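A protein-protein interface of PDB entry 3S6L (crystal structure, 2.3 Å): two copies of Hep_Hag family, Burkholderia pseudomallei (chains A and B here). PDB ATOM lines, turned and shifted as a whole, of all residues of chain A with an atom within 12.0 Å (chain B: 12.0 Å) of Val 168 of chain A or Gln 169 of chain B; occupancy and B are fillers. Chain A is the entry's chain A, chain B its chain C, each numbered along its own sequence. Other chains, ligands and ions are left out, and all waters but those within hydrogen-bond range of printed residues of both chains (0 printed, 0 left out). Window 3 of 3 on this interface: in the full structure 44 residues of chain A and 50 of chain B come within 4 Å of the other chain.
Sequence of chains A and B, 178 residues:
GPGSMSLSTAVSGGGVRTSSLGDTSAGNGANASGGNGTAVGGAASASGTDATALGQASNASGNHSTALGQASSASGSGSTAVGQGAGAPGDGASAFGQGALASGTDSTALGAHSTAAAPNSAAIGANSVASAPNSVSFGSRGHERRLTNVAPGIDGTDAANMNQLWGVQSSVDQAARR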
ATOM      1  N   PRO A 152      13.075  -3.043 -39.239  1.00  0.00           N
ATOM      2  CA  PRO A 152      13.292  -3.149 -37.788  1.00  0.00           C
ATOM      3  C   PRO A 152      14.711  -3.655 -37.484  1.00  0.00           C
ATOM      4  O   PRO A 152      15.244  -4.515 -38.205  1.00  0.00           O
ATOM      5  CB  PRO A 152      12.208  -4.137 -37.334  1.00  0.00           C
ATOM      6  CG  PRO A 152      11.833  -4.916 -38.540  1.00  0.00           C
ATOM      7  CD  PRO A 152      12.180  -4.108 -39.756  1.00  0.00           C
ATOM      8  N   GLY A 153      15.337  -3.086 -36.456  1.00  0.00           N
ATOM      9  CA  GLY A 153      16.682  -3.486 -36.084  1.00  0.00           C
ATOM     10  C   GLY A 153      16.790  -4.909 -35.558  1.00  0.00           C
ATOM     11  O   GLY A 153      15.853  -5.453 -34.941  1.00  0.00           O
ATOM     12  N   ALA A 159      19.501   0.655 -35.674  1.00  0.00           N
ATOM     13  CA  ALA A 159      18.427   1.573 -35.290  1.00  0.00           C
ATOM     14  C   ALA A 159      17.101   0.842 -34.959  1.00  0.00           C
ATOM     15  O   ALA A 159      16.767  -0.196 -35.568  1.00  0.00           O
ATOM     16  CB  ALA A 159      18.189   2.605 -36.389  1.00  0.00           C
ATOM     17  N   ALA A 160      16.365   1.392 -33.988  1.00  0.00           N
ATOM     18  CA  ALA A 160      15.029   0.917 -33.642  1.00  0.00           C
ATOM     19  C   ALA A 160      14.026   1.728 -34.441  1.00  0.00           C
ATOM     20  O   ALA A 160      14.101   2.965 -34.476  1.00  0.00           O
ATOM     21  CB  ALA A 160      14.752   1.081 -32.134  1.00  0.00           C
ATOM     22  N   ASN A 161      13.075   1.048 -35.082  1.00  0.00           N
ATOM     23  CA  ASN A 161      12.004   1.786 -35.740  1.00  0.00           C
ATOM     24  C   ASN A 161      10.778   1.898 -34.828  1.00  0.00           C
ATOM     25  O   ASN A 161      10.763   1.308 -33.731  1.00  0.00           O
ATOM     26  CB  ASN A 161      11.703   1.230 -37.138  1.00  0.00           C
ATOM     27  CG  ASN A 161      10.845  -0.025 -37.112  1.00  0.00           C
ATOM     28  OD1 ASN A 161      10.273  -0.392 -36.093  1.00  0.00           O
ATOM     29  ND2 ASN A 161      10.733  -0.660 -38.244  1.00  0.00           N
ATOM     30  N   MET A 162       9.766   2.651 -35.271  1.00  0.00           N
ATOM     31  CA  MET A 162       8.591   2.958 -34.457  1.00  0.00           C
ATOM     32  C   MET A 162       7.750   1.729 -34.098  1.00  0.00           C
ATOM     33  O   MET A 162       7.253   1.642 -32.981  1.00  0.00           O
ATOM     34  CB  MET A 162       7.702   4.007 -35.137  1.00  0.00           C
ATOM     35  CG  MET A 162       8.241   5.456 -35.158  1.00  0.00           C
ATOM     36  SD  MET A 162       8.832   6.073 -33.579  1.00  0.00           S
ATOM     37  CE  MET A 162       7.329   6.099 -32.558  1.00  0.00           C
ATOM     38  N   ASN A 163       7.570   0.801 -35.037  1.00  0.00           N
ATOM     39  CA  ASN A 163       6.869  -0.457 -34.741  1.00  0.00           C
ATOM     40  C   ASN A 163       7.483  -1.139 -33.520  1.00  0.00           C
ATOM     41  O   ASN A 163       6.766  -1.660 -32.662  1.00  0.00           O
ATOM     42  CB  ASN A 163       6.889  -1.410 -35.937  1.00  0.00           C
ATOM     43  CG  ASN A 163       5.895  -1.015 -37.027  1.00  0.00           C
ATOM     44  OD1 ASN A 163       4.808  -0.523 -36.732  1.00  0.00           O
ATOM     45  ND2 ASN A 163       6.263  -1.235 -38.295  1.00  0.00           N
ATOM     46  N   GLN A 164       8.814  -1.110 -33.439  1.00  0.00           N
ATOM     47  CA  GLN A 164       9.524  -1.753 -32.350  1.00  0.00           C
ATOM     48  C   GLN A 164       9.332  -0.984 -31.050  1.00  0.00           C
ATOM     49  O   GLN A 164       9.139  -1.595 -29.991  1.00  0.00           O
ATOM     50  CB  GLN A 164      10.997  -1.931 -32.685  1.00  0.00           C
ATOM     51  CG  GLN A 164      11.238  -2.735 -33.943  1.00  0.00           C
ATOM     52  CD  GLN A 164      12.697  -2.862 -34.247  1.00  0.00           C
ATOM     53  OE1 GLN A 164      13.347  -1.887 -34.630  1.00  0.00           O
ATOM     54  NE2 GLN A 164      13.242  -4.072 -34.070  1.00  0.00           N
ATOM     55  N   LEU A 165       9.373   0.345 -31.128  1.00  0.00           N
ATOM     56  CA  LEU A 165       9.140   1.174 -29.958  1.00  0.00           C
ATOM     57  C   LEU A 165       7.740   0.902 -29.379  1.00  0.00           C
ATOM     58  O   LEU A 165       7.598   0.637 -28.195  1.00  0.00           O
ATOM     59  CB  LEU A 165       9.305   2.660 -30.297  1.00  0.00           C
ATOM     60  CG  LEU A 165       9.365   3.578 -29.074  1.00  0.00           C
ATOM     61  CD1 LEU A 165      10.779   3.657 -28.547  1.00  0.00           C
ATOM     62  CD2 LEU A 165       8.857   4.961 -29.390  1.00  0.00           C
ATOM     63  N   TRP A 166       6.728   0.958 -30.238  1.00  0.00           N
ATOM     64  CA  TRP A 166       5.352   0.642 -29.886  1.00  0.00           C
ATOM     65  C   TRP A 166       5.105  -0.779 -29.359  1.00  0.00           C
ATOM     66  O   TRP A 166       4.173  -1.003 -28.591  1.00  0.00           O
ATOM     67  CB  TRP A 166       4.463   0.878 -31.085  1.00  0.00           C
ATOM     68  CG  TRP A 166       4.429   2.301 -31.550  1.00  0.00           C
ATOM     69  CD1 TRP A 166       4.638   3.433 -30.797  1.00  0.00           C
ATOM     70  CD2 TRP A 166       4.099   2.752 -32.870  1.00  0.00           C
ATOM     71  NE1 TRP A 166       4.465   4.547 -31.578  1.00  0.00           N
ATOM     72  CE2 TRP A 166       4.131   4.159 -32.851  1.00  0.00           C
ATOM     73  CE3 TRP A 166       3.759   2.097 -34.066  1.00  0.00           C
ATOM     74  CZ2 TRP A 166       3.858   4.925 -33.985  1.00  0.00           C
ATOM     75  CZ3 TRP A 166       3.490   2.860 -35.195  1.00  0.00           C
ATOM     76  CH2 TRP A 166       3.537   4.258 -35.144  1.00  0.00           C
ATOM     77  N   GLY A 167       5.934  -1.730 -29.784  1.00  0.00           N
ATOM     78  CA  GLY A 167       5.881  -3.102 -29.272  1.00  0.00           C
ATOM     79  C   GLY A 167       6.351  -3.195 -27.830  1.00  0.00           C
ATOM     80  O   GLY A 167       6.068  -4.176 -27.147  1.00  0.00           O
ATOM     81  N   VAL A 168       7.075  -2.176 -27.368  1.00  0.00           N
ATOM     82  CA  VAL A 168       7.463  -2.075 -25.961  1.00  0.00           C
ATOM     83  C   VAL A 168       6.354  -1.369 -25.173  1.00  0.00           C
ATOM     84  O   VAL A 168       5.907  -1.877 -24.133  1.00  0.00           O
ATOM     85  CB  VAL A 168       8.838  -1.364 -25.779  1.00  0.00           C
ATOM     86  CG1 VAL A 168       9.184  -1.195 -24.286  1.00  0.00           C
ATOM     87  CG2 VAL A 168       9.935  -2.145 -26.508  1.00  0.00           C
ATOM     88  N   GLN A 169       5.896  -0.226 -25.696  1.00  0.00           N
ATOM     89  CA  GLN A 169       4.755   0.528 -25.148  1.00  0.00           C
ATOM     90  C   GLN A 169       3.524  -0.347 -24.785  1.00  0.00           C
ATOM     91  O   GLN A 169       2.570   0.142 -24.162  1.00  0.00           O
ATOM     92  CB  GLN A 169       4.364   1.687 -26.093  1.00  0.00           C
ATOM     93  N   SER A 170       3.555  -1.625 -25.177  1.00  0.00           N
ATOM     94  CA  SER A 170       2.575  -2.615 -24.718  1.00  0.00           C
ATOM     95  C   SER A 170       3.254  -3.947 -24.367  1.00  0.00           C
ATOM     96  O   SER A 170       3.541  -4.227 -23.198  1.00  0.00           O
ATOM     97  CB  SER A 170       1.482  -2.828 -25.774  1.00  0.00           C
ATOM     98  OG  SER A 170       0.368  -3.528 -25.224  1.00  0.00           O
ATOM     99  N   ALA B 160      17.718   6.155 -31.587  1.00  0.00           N
ATOM    100  CA  ALA B 160      17.829   5.127 -30.556  1.00  0.00           C
ATOM    101  C   ALA B 160      18.230   3.819 -31.226  1.00  0.00           C
ATOM    102  O   ALA B 160      17.623   3.454 -32.235  1.00  0.00           O
ATOM    103  CB  ALA B 160      16.478   4.956 -29.863  1.00  0.00           C
ATOM    104  N   ASN B 161      19.221   3.099 -30.688  1.00  0.00           N
ATOM    105  CA  ASN B 161      19.524   1.769 -31.234  1.00  0.00           C
ATOM    106  C   ASN B 161      18.868   0.604 -30.468  1.00  0.00           C
ATOM    107  O   ASN B 161      18.170   0.820 -29.470  1.00  0.00           O
ATOM    108  CB  ASN B 161      21.032   1.565 -31.430  1.00  0.00           C
ATOM    109  CG  ASN B 161      21.773   1.327 -30.127  1.00  0.00           C
ATOM    110  OD1 ASN B 161      21.155   1.084 -29.083  1.00  0.00           O
ATOM    111  ND2 ASN B 161      23.115   1.387 -30.183  1.00  0.00           N
ATOM    112  N   MET B 162      19.090  -0.625 -30.932  1.00  0.00           N
ATOM    113  CA  MET B 162      18.365  -1.768 -30.366  1.00  0.00           C
ATOM    114  C   MET B 162      18.796  -2.040 -28.924  1.00  0.00           C
ATOM    115  O   MET B 162      17.952  -2.271 -28.064  1.00  0.00           O
ATOM    116  CB  MET B 162      18.470  -3.018 -31.253  1.00  0.00           C
ATOM    117  CG  MET B 162      17.673  -2.965 -32.561  1.00  0.00           C
ATOM    118  SD  MET B 162      15.907  -2.615 -32.407  1.00  0.00           S
ATOM    119  CE  MET B 162      15.389  -3.923 -31.284  1.00  0.00           C
ATOM    120  N   ASN B 163      20.090  -1.936 -28.646  1.00  0.00           N
ATOM    121  CA  ASN B 163      20.598  -2.028 -27.273  1.00  0.00           C
ATOM    122  C   ASN B 163      19.870  -1.094 -26.323  1.00  0.00           C
ATOM    123  O   ASN B 163      19.540  -1.487 -25.208  1.00  0.00           O
ATOM    124  CB  ASN B 163      22.103  -1.752 -27.214  1.00  0.00           C
ATOM    125  CG  ASN B 163      22.936  -2.957 -27.568  1.00  0.00           C
ATOM    126  OD1 ASN B 163      22.518  -4.103 -27.359  1.00  0.00           O
ATOM    127  ND2 ASN B 163      24.135  -2.711 -28.115  1.00  0.00           N
ATOM    128  N   GLN B 164      19.618   0.143 -26.745  1.00  0.00           N
ATOM    129  CA  GLN B 164      18.878   1.063 -25.891  1.00  0.00           C
ATOM    130  C   GLN B 164      17.415   0.643 -25.798  1.00  0.00           C
ATOM    131  O   GLN B 164      16.823   0.714 -24.724  1.00  0.00           O
ATOM    132  CB  GLN B 164      19.007   2.519 -26.363  1.00  0.00           C
ATOM    133  CG  GLN B 164      20.437   3.074 -26.334  1.00  0.00           C
ATOM    134  CD  GLN B 164      20.587   4.370 -27.125  1.00  0.00           C
ATOM    135  OE1 GLN B 164      20.398   4.398 -28.354  1.00  0.00           O
ATOM    136  NE2 GLN B 164      20.943   5.451 -26.423  1.00  0.00           N
ATOM    137  N   LEU B 165      16.829   0.213 -26.909  1.00  0.00           N
ATOM    138  CA  LEU B 165      15.445  -0.257 -26.873  1.00  0.00           C
ATOM    139  C   LEU B 165      15.293  -1.477 -25.938  1.00  0.00           C
ATOM    140  O   LEU B 165      14.313  -1.567 -25.207  1.00  0.00           O
ATOM    141  CB  LEU B 165      14.869  -0.551 -28.280  1.00  0.00           C
ATOM    142  CG  LEU B 165      13.390  -0.983 -28.258  1.00  0.00           C
ATOM    143  CD1 LEU B 165      12.481   0.206 -27.950  1.00  0.00           C
ATOM    144  CD2 LEU B 165      12.917  -1.680 -29.503  1.00  0.00           C
ATOM    145  N   TRP B 166      16.271  -2.383 -25.947  1.00  0.00           N
ATOM    146  CA  TRP B 166      16.235  -3.562 -25.077  1.00  0.00           C
ATOM    147  C   TRP B 166      16.358  -3.238 -23.593  1.00  0.00           C
ATOM    148  O   TRP B 166      15.664  -3.847 -22.770  1.00  0.00           O
ATOM    149  CB  TRP B 166      17.285  -4.590 -25.477  1.00  0.00           C
ATOM    150  CG  TRP B 166      16.993  -5.214 -26.791  1.00  0.00           C
ATOM    151  CD1 TRP B 166      15.755  -5.467 -27.323  1.00  0.00           C
ATOM    152  CD2 TRP B 166      17.948  -5.687 -27.752  1.00  0.00           C
ATOM    153  NE1 TRP B 166      15.883  -6.063 -28.548  1.00  0.00           N
ATOM    154  CE2 TRP B 166      17.216  -6.214 -28.839  1.00  0.00           C
ATOM    155  CE3 TRP B 166      19.351  -5.737 -27.789  1.00  0.00           C
ATOM    156  CZ2 TRP B 166      17.837  -6.766 -29.966  1.00  0.00           C
ATOM    157  CZ3 TRP B 166      19.971  -6.287 -28.906  1.00  0.00           C
ATOM    158  CH2 TRP B 166      19.211  -6.790 -29.983  1.00  0.00           C
ATOM    159  N   GLY B 167      17.225  -2.279 -23.263  1.00  0.00           N
ATOM    160  CA  GLY B 167      17.385  -1.808 -21.895  1.00  0.00           C
ATOM    161  C   GLY B 167      16.143  -1.120 -21.354  1.00  0.00           C
ATOM    162  O   GLY B 167      15.937  -1.059 -20.133  1.00  0.00           O
ATOM    163  N   VAL B 168      15.311  -0.599 -22.260  1.00  0.00           N
ATOM    164  CA  VAL B 168      14.022  -0.024 -21.869  1.00  0.00           C
ATOM    165  C   VAL B 168      12.930  -1.084 -21.708  1.00  0.00           C
ATOM    166  O   VAL B 168      12.060  -0.945 -20.849  1.00  0.00           O
ATOM    167  CB  VAL B 168      13.602   1.136 -22.795  1.00  0.00           C
ATOM    168  CG1 VAL B 168      12.100   1.402 -22.729  1.00  0.00           C
ATOM    169  CG2 VAL B 168      14.381   2.392 -22.409  1.00  0.00           C
ATOM    170  N   GLN B 169      12.994  -2.153 -22.505  1.00  0.00           N
ATOM    171  CA  GLN B 169      12.078  -3.302 -22.347  1.00  0.00           C
ATOM    172  C   GLN B 169      12.299  -4.076 -21.015  1.00  0.00           C
ATOM    173  O   GLN B 169      11.812  -5.195 -20.851  1.00  0.00           O
ATOM    174  CB  GLN B 169      12.168  -4.223 -23.582  1.00  0.00           C
ATOM    175  CG  GLN B 169      11.311  -5.504 -23.546  1.00  0.00           C
ATOM    176  CD  GLN B 169       9.971  -5.387 -24.271  1.00  0.00           C
ATOM    177  OE1 GLN B 169       9.923  -5.276 -25.500  1.00  0.00           O
ATOM    178  NE2 GLN B 169       8.876  -5.457 -23.513  1.00  0.00           N
ATOM    179  N   SER B 170      12.995  -3.458 -20.054  1.00  0.00           N
ATOM    180  CA  SER B 170      13.257  -4.085 -18.747  1.00  0.00           C
ATOM    181  C   SER B 170      12.685  -3.307 -17.543  1.00  0.00           C
ATOM    182  O   SER B 170      12.775  -2.072 -17.457  1.00  0.00           O
ATOM    183  CB  SER B 170      14.761  -4.357 -18.585  1.00  0.00           C
ATOM    184  OG  SER B 170      15.253  -5.163 -19.654  1.00  0.00           O
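The backbone NH (N) of Gly 153 of chain A sits close to the backbone carbonyl oxygen (O) of Ala 159 of chain A (3.3 Å).
The backbone NH (N) of Gly 153 of chain A lies within hydrogen-bond range of the side-chain amide oxygen (OE1) of Gln 164 of chain A.
The backbone NH (N) of Asn 161 of chain A lies within hydrogen-bond range of the side-chain amide oxygen (OE1) of Gln 164 of chain A, 3.0 Å away.
Ala 160 of chain B touches its own counterpart, Ala 160 of chain A.
Ala 160 of chain A touches Met 162 of chain B, but with the chains exchanged Met 162 of chain A does not touch Ala 160 of chain B (8.5 Å).
Gln 164 of chain A touches Met 162 of chain B, but with the chains exchanged Met 162 of chain A does not touch Gln 164 of chain B (12.3 Å).
Leu 165 of chain B touches its own counterpart, Leu 165 of chain A.
Positions printed for both chains: 160, 161, 162, 163, 164, 165, 166, 167, 168, 169 and 170.
Hydrophobic or aromatic side chains of chain B within 4 Å of the printed part of chain A: Met 162 and Leu 165.
Of the 14 printed residues of chain A, 6 touch a printed residue of chain B.
Among the printed residues, 9 pairs touch across the chains.
Among the printed residues, no Asp or Glu carboxylate lies within 4 Å of a Lys or Arg side-chain nitrogen of the other chain.
The backbone NH (N) of Ala 160 of chain A sits at hydrogen-bond distance from the backbone carbonyl oxygen (O) of Ala 160 of chain B.
The side-chain amide nitrogen of Gln 164 of chain A lies within hydrogen-bond range of the side-chain sulfur of Met 162 of chain B.
Printed residues of chain B within 4 Å of Ala 159 of chain A: Ala 160.
Of the printed residues of chain B, Ala 160 of chain A touches Ala 160 (3.0 Å) and Met 162 (3.8 Å).
Of chain B, only Leu 165 (3.8 Å) and Gln 169 (3.3 Å) come within 4 Å of Val 168 of chain A.
Of the printed residues of chain A, Ala 160 of chain B touches Ala 159 (3.7 Å) and Ala 160 (3.0 Å).
Asn 161 of chain B touches none of the printed residues of chain A.
Of chain A, only Gln 164, Leu 165 and Val 168 come within 4 Å of Leu 165 of chain B.
No residue of chain A comes within 4 Å of Val 168 of chain B.
The nearest residue of chain B that does not touch Val 168 of chain A is Val 168 of chain B (4.2 Å).
CG of Met 162 of chain B touches C of Gly 153 of chain A (3.7 Å).
Ala 159 of chain A touches Ala 160 of chain B.
Ala 160 of chain A touches Met 162 of chain B.
CB of Gln 164 of chain A touches CD2 of Leu 165 of chain B, 3.7 Å away.
Leu 165 of chain A touches Leu 165 of chain B.
Val 168 of chain A touches Leu 165 of chain B (CG2 to CD1, 3.8 Å).
Gln 169 of chain B touches Val 168 of chain A.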
